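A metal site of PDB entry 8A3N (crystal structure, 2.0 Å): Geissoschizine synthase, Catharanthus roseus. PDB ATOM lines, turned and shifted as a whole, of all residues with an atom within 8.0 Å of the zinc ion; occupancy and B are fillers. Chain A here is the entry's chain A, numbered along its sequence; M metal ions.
N of Gln 107 lies close to SG of Cys 105.
The backbone NH of Glu 121 sits close to the side-chain sulfur of Cys 119, at 3.3 Å.
The side-chain sulfur (SG) of Cys 111 lies close to the backbone NH (N) of Gly 106 (3.3 Å).
SG of Cys 111 sits close to OG of Ser 104 (3.1 Å).
The side-chain sulfur (SG) of Cys 108 lies close to the backbone NH (N) of Asn 110 (3.6 Å).
The zinc ion is bound by the side-chain sulfur (SG) of Cys 105, at 2.3 Å.
SG of Cys 119 binds the zinc ion (2.3 Å).
The zinc ion is bound by SG of Cys 111, at 2.3 Å.
The zinc ion is bound by SG of Cys 108.
The zinc ion has four donor atoms within binding distance.
Gly 106 touches the zinc ion (N to ZN, 3.7 Å).
Within 4 Å of the zinc ion: Cys 105, Gly 106, Cys 108, Cys 111 and Cys 119.
The nearest printed residue that does not touch the zinc ion is Pro 120 (4.1 Å).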
ATOM      1  N   MET A 101     -19.751 -20.602  13.416  1.00  0.00           N
ATOM      2  CA  MET A 101     -20.858 -20.352  14.322  1.00  0.00           C
ATOM      3  C   MET A 101     -21.966 -21.393  14.164  1.00  0.00           C
ATOM      4  O   MET A 101     -22.187 -21.883  13.062  1.00  0.00           O
ATOM      5  CB  MET A 101     -21.461 -18.973  14.057  1.00  0.00           C
ATOM      6  CG  MET A 101     -20.555 -17.856  14.546  1.00  0.00           C
ATOM      7  SD  MET A 101     -21.268 -16.253  14.159  1.00  0.00           S
ATOM      8  CE  MET A 101     -22.564 -16.192  15.404  1.00  0.00           C
ATOM      9  N   GLY A 103     -24.899 -20.650  16.239  1.00  0.00           N
ATOM     10  CA  GLY A 103     -26.026 -19.933  16.820  1.00  0.00           C
ATOM     11  C   GLY A 103     -25.695 -18.470  17.050  1.00  0.00           C
ATOM     12  O   GLY A 103     -24.527 -18.080  17.024  1.00  0.00           O
ATOM     13  N   SER A 104     -26.745 -17.675  17.236  1.00  0.00           N
ATOM     14  CA  SER A 104     -26.625 -16.279  17.607  1.00  0.00           C
ATOM     15  C   SER A 104     -27.928 -15.861  18.290  1.00  0.00           C
ATOM     16  O   SER A 104     -28.842 -16.669  18.375  1.00  0.00           O
ATOM     17  CB  SER A 104     -26.295 -15.414  16.399  1.00  0.00           C
ATOM     18  OG  SER A 104     -27.397 -15.311  15.500  1.00  0.00           O
ATOM     19  N   CYS A 105     -27.984 -14.626  18.798  1.00  0.00           N
ATOM     20  CA  CYS A 105     -29.147 -14.201  19.578  1.00  0.00           C
ATOM     21  C   CYS A 105     -30.379 -14.144  18.672  1.00  0.00           C
ATOM     22  O   CYS A 105     -31.493 -14.405  19.135  1.00  0.00           O
ATOM     23  CB  CYS A 105     -28.901 -12.879  20.295  1.00  0.00           C
ATOM     24  SG  CYS A 105     -29.261 -11.410  19.303  1.00  0.00           S
ATOM     25  N   GLY A 106     -30.194 -13.763  17.407  1.00  0.00           N
ATOM     26  CA  GLY A 106     -31.255 -13.798  16.418  1.00  0.00           C
ATOM     27  C   GLY A 106     -32.217 -12.609  16.471  1.00  0.00           C
ATOM     28  O   GLY A 106     -33.160 -12.554  15.689  1.00  0.00           O
ATOM     29  N   GLN A 107     -31.984 -11.640  17.381  1.00  0.00           N
ATOM     30  CA  GLN A 107     -32.912 -10.530  17.558  1.00  0.00           C
ATOM     31  C   GLN A 107     -32.201  -9.169  17.522  1.00  0.00           C
ATOM     32  O   GLN A 107     -32.885  -8.138  17.528  1.00  0.00           O
ATOM     33  CB  GLN A 107     -33.710 -10.706  18.845  1.00  0.00           C
ATOM     34  CG  GLN A 107     -32.908 -10.427  20.111  1.00  0.00           C
ATOM     35  CD  GLN A 107     -33.618 -10.883  21.370  1.00  0.00           C
ATOM     36  OE1 GLN A 107     -33.779 -12.074  21.613  1.00  0.00           O
ATOM     37  NE2 GLN A 107     -34.032  -9.927  22.186  1.00  0.00           N
ATOM     38  N   CYS A 108     -30.870  -9.135  17.501  1.00  0.00           N
ATOM     39  CA  CYS A 108     -30.132  -7.868  17.446  1.00  0.00           C
ATOM     40  C   CYS A 108     -30.086  -7.381  16.001  1.00  0.00           C
ATOM     41  O   CYS A 108     -30.342  -8.141  15.071  1.00  0.00           O
ATOM     42  CB  CYS A 108     -28.736  -7.997  18.039  1.00  0.00           C
ATOM     43  SG  CYS A 108     -27.552  -8.918  17.014  1.00  0.00           S
ATOM     44  N   TYR A 109     -29.730  -6.104  15.815  1.00  0.00           N
ATOM     45  CA  TYR A 109     -29.679  -5.509  14.486  1.00  0.00           C
ATOM     46  C   TYR A 109     -28.736  -6.319  13.573  1.00  0.00           C
ATOM     47  O   TYR A 109     -29.023  -6.506  12.396  1.00  0.00           O
ATOM     48  CB  TYR A 109     -29.254  -4.032  14.549  1.00  0.00           C
ATOM     49  CG  TYR A 109     -29.044  -3.397  13.202  1.00  0.00           C
ATOM     50  CD1 TYR A 109     -30.103  -2.995  12.402  1.00  0.00           C
ATOM     51  CD2 TYR A 109     -27.755  -3.245  12.690  1.00  0.00           C
ATOM     52  CE1 TYR A 109     -29.904  -2.447  11.145  1.00  0.00           C
ATOM     53  CE2 TYR A 109     -27.540  -2.708  11.438  1.00  0.00           C
ATOM     54  CZ  TYR A 109     -28.614  -2.301  10.657  1.00  0.00           C
ATOM     55  OH  TYR A 109     -28.352  -1.760   9.425  1.00  0.00           O
ATOM     56  N   ASN A 110     -27.608  -6.777  14.125  1.00  0.00           N
ATOM     57  CA  ASN A 110     -26.631  -7.508  13.330  1.00  0.00           C
ATOM     58  C   ASN A 110     -27.230  -8.816  12.836  1.00  0.00           C
ATOM     59  O   ASN A 110     -27.104  -9.130  11.652  1.00  0.00           O
ATOM     60  CB  ASN A 110     -25.337  -7.757  14.119  1.00  0.00           C
ATOM     61  CG  ASN A 110     -24.565  -6.486  14.352  1.00  0.00           C
ATOM     62  OD1 ASN A 110     -24.491  -5.651  13.447  1.00  0.00           O
ATOM     63  ND2 ASN A 110     -24.005  -6.313  15.546  1.00  0.00           N
ATOM     64  N   CYS A 111     -27.880  -9.564  13.736  1.00  0.00           N
ATOM     65  CA  CYS A 111     -28.522 -10.821  13.385  1.00  0.00           C
ATOM     66  C   CYS A 111     -29.615 -10.602  12.344  1.00  0.00           C
ATOM     67  O   CYS A 111     -29.705 -11.340  11.365  1.00  0.00           O
ATOM     68  CB  CYS A 111     -29.077 -11.507  14.634  1.00  0.00           C
ATOM     69  SG  CYS A 111     -27.799 -12.269  15.673  1.00  0.00           S
ATOM     70  N   GLN A 112     -30.440  -9.558  12.526  1.00  0.00           N
ATOM     71  CA  GLN A 112     -31.543  -9.243  11.623  1.00  0.00           C
ATOM     72  C   GLN A 112     -31.025  -8.902  10.227  1.00  0.00           C
ATOM     73  O   GLN A 112     -31.672  -9.241   9.242  1.00  0.00           O
ATOM     74  CB  GLN A 112     -32.339  -8.052  12.156  1.00  0.00           C
ATOM     75  CG  GLN A 112     -32.981  -8.279  13.519  1.00  0.00           C
ATOM     76  CD  GLN A 112     -34.278  -9.039  13.442  1.00  0.00           C
ATOM     77  OE1 GLN A 112     -34.307 -10.241  13.186  1.00  0.00           O
ATOM     78  NE2 GLN A 112     -35.378  -8.339  13.702  1.00  0.00           N
ATOM     79  N   MET A 115     -25.732 -10.376   9.650  1.00  0.00           N
ATOM     80  CA  MET A 115     -24.342 -10.276  10.074  1.00  0.00           C
ATOM     81  C   MET A 115     -24.181 -10.924  11.449  1.00  0.00           C
ATOM     82  O   MET A 115     -23.755 -10.284  12.413  1.00  0.00           O
ATOM     83  CB  MET A 115     -23.889  -8.804  10.113  1.00  0.00           C
ATOM     84  CG  MET A 115     -23.715  -8.184   8.721  1.00  0.00           C
ATOM     85  SD  MET A 115     -22.947  -9.280   7.455  1.00  0.00           S
ATOM     86  CE  MET A 115     -21.332  -9.563   8.175  1.00  0.00           C
ATOM     87  N   GLU A 116     -24.501 -12.214  11.519  1.00  0.00           N
ATOM     88  CA  GLU A 116     -24.567 -12.949  12.775  1.00  0.00           C
ATOM     89  C   GLU A 116     -23.184 -13.046  13.403  1.00  0.00           C
ATOM     90  O   GLU A 116     -23.063 -13.157  14.611  1.00  0.00           O
ATOM     91  CB  GLU A 116     -25.140 -14.353  12.575  1.00  0.00           C
ATOM     92  CG  GLU A 116     -26.493 -14.382  11.884  1.00  0.00           C
ATOM     93  CD  GLU A 116     -26.463 -14.291  10.357  1.00  0.00           C
ATOM     94  OE1 GLU A 116     -25.343 -14.154   9.790  1.00  0.00           O
ATOM     95  OE2 GLU A 116     -27.558 -14.367   9.746  1.00  0.00           O
ATOM     96  N   ASN A 117     -22.139 -12.976  12.579  1.00  0.00           N
ATOM     97  CA  ASN A 117     -20.771 -13.010  13.060  1.00  0.00           C
ATOM     98  C   ASN A 117     -20.461 -11.804  13.927  1.00  0.00           C
ATOM     99  O   ASN A 117     -19.487 -11.817  14.659  1.00  0.00           O
ATOM    100  CB  ASN A 117     -19.776 -13.167  11.893  1.00  0.00           C
ATOM    101  CG  ASN A 117     -19.893 -12.097  10.831  1.00  0.00           C
ATOM    102  OD1 ASN A 117     -20.993 -11.660  10.485  1.00  0.00           O
ATOM    103  ND2 ASN A 117     -18.779 -11.670  10.287  1.00  0.00           N
ATOM    104  N   TYR A 118     -21.279 -10.745  13.858  1.00  0.00           N
ATOM    105  CA  TYR A 118     -21.094  -9.581  14.712  1.00  0.00           C
ATOM    106  C   TYR A 118     -22.215  -9.465  15.733  1.00  0.00           C
ATOM    107  O   TYR A 118     -22.463  -8.386  16.266  1.00  0.00           O
ATOM    108  CB  TYR A 118     -20.960  -8.316  13.858  1.00  0.00           C
ATOM    109  CG  TYR A 118     -19.741  -8.310  12.968  1.00  0.00           C
ATOM    110  CD1 TYR A 118     -18.472  -8.178  13.501  1.00  0.00           C
ATOM    111  CD2 TYR A 118     -19.863  -8.485  11.590  1.00  0.00           C
ATOM    112  CE1 TYR A 118     -17.349  -8.190  12.683  1.00  0.00           C
ATOM    113  CE2 TYR A 118     -18.748  -8.492  10.770  1.00  0.00           C
ATOM    114  CZ  TYR A 118     -17.493  -8.354  11.322  1.00  0.00           C
ATOM    115  OH  TYR A 118     -16.390  -8.380  10.498  1.00  0.00           O
ATOM    116  N   CYS A 119     -22.882 -10.585  16.035  1.00  0.00           N
ATOM    117  CA  CYS A 119     -23.785 -10.651  17.168  1.00  0.00           C
ATOM    118  C   CYS A 119     -22.968 -10.488  18.447  1.00  0.00           C
ATOM    119  O   CYS A 119     -21.887 -11.064  18.559  1.00  0.00           O
ATOM    120  CB  CYS A 119     -24.513 -11.981  17.209  1.00  0.00           C
ATOM    121  SG  CYS A 119     -25.673 -12.132  18.598  1.00  0.00           S
ATOM    122  N   PRO A 120     -23.446  -9.725  19.458  1.00  0.00           N
ATOM    123  CA  PRO A 120     -22.783  -9.666  20.763  1.00  0.00           C
ATOM    124  C   PRO A 120     -22.667 -11.028  21.465  1.00  0.00           C
ATOM    125  O   PRO A 120     -21.772 -11.211  22.277  1.00  0.00           O
ATOM    126  CB  PRO A 120     -23.678  -8.758  21.616  1.00  0.00           C
ATOM    127  CG  PRO A 120     -24.496  -7.969  20.607  1.00  0.00           C
ATOM    128  CD  PRO A 120     -24.639  -8.872  19.410  1.00  0.00           C
ATOM    129  N   GLU A 121     -23.580 -11.958  21.154  1.00  0.00           N
ATOM    130  CA  GLU A 121     -23.664 -13.238  21.835  1.00  0.00           C
ATOM    131  C   GLU A 121     -23.566 -14.383  20.824  1.00  0.00           C
ATOM    132  O   GLU A 121     -24.521 -15.125  20.640  1.00  0.00           O
ATOM    133  CB  GLU A 121     -24.985 -13.352  22.597  1.00  0.00           C
ATOM    134  CG  GLU A 121     -25.309 -12.179  23.501  1.00  0.00           C
ATOM    135  CD  GLU A 121     -26.643 -12.335  24.205  1.00  0.00           C
ATOM    136  OE1 GLU A 121     -27.562 -11.518  23.937  1.00  0.00           O
ATOM    137  OE2 GLU A 121     -26.775 -13.272  25.016  1.00  0.00           O
ATOM    138  N   PRO A 122     -22.423 -14.555  20.117  1.00  0.00           N
ATOM    139  CA  PRO A 122     -22.285 -15.644  19.149  1.00  0.00           C
ATOM    140  C   PRO A 122     -22.148 -16.983  19.879  1.00  0.00           C
ATOM    141  O   PRO A 122     -21.612 -17.042  20.982  1.00  0.00           O
ATOM    142  CB  PRO A 122     -21.029 -15.256  18.362  1.00  0.00           C
ATOM    143  CG  PRO A 122     -20.208 -14.454  19.347  1.00  0.00           C
ATOM    144  CD  PRO A 122     -21.198 -13.753  20.248  1.00  0.00           C
ATOM    145  N   LYS A 150     -30.301 -23.014  10.310  1.00  0.00           N
ATOM    146  CA  LYS A 150     -29.965 -21.659   9.944  1.00  0.00           C
ATOM    147  C   LYS A 150     -28.459 -21.521   9.740  1.00  0.00           C
ATOM    148  O   LYS A 150     -28.039 -20.737   8.905  1.00  0.00           O
ATOM    149  CB  LYS A 150     -30.470 -20.668  10.996  1.00  0.00           C
ATOM    150  CG  LYS A 150     -30.117 -19.216  10.720  1.00  0.00           C
ATOM    151  CD  LYS A 150     -30.696 -18.216  11.702  1.00  0.00           C
ATOM    152  CE  LYS A 150     -30.240 -16.809  11.390  1.00  0.00           C
ATOM    153  NZ  LYS A 150     -30.920 -15.819  12.260  1.00  0.00           N
HETATM  154 ZN    ZN M   1     -27.599 -11.156  17.722  1.00  0.00          ZN
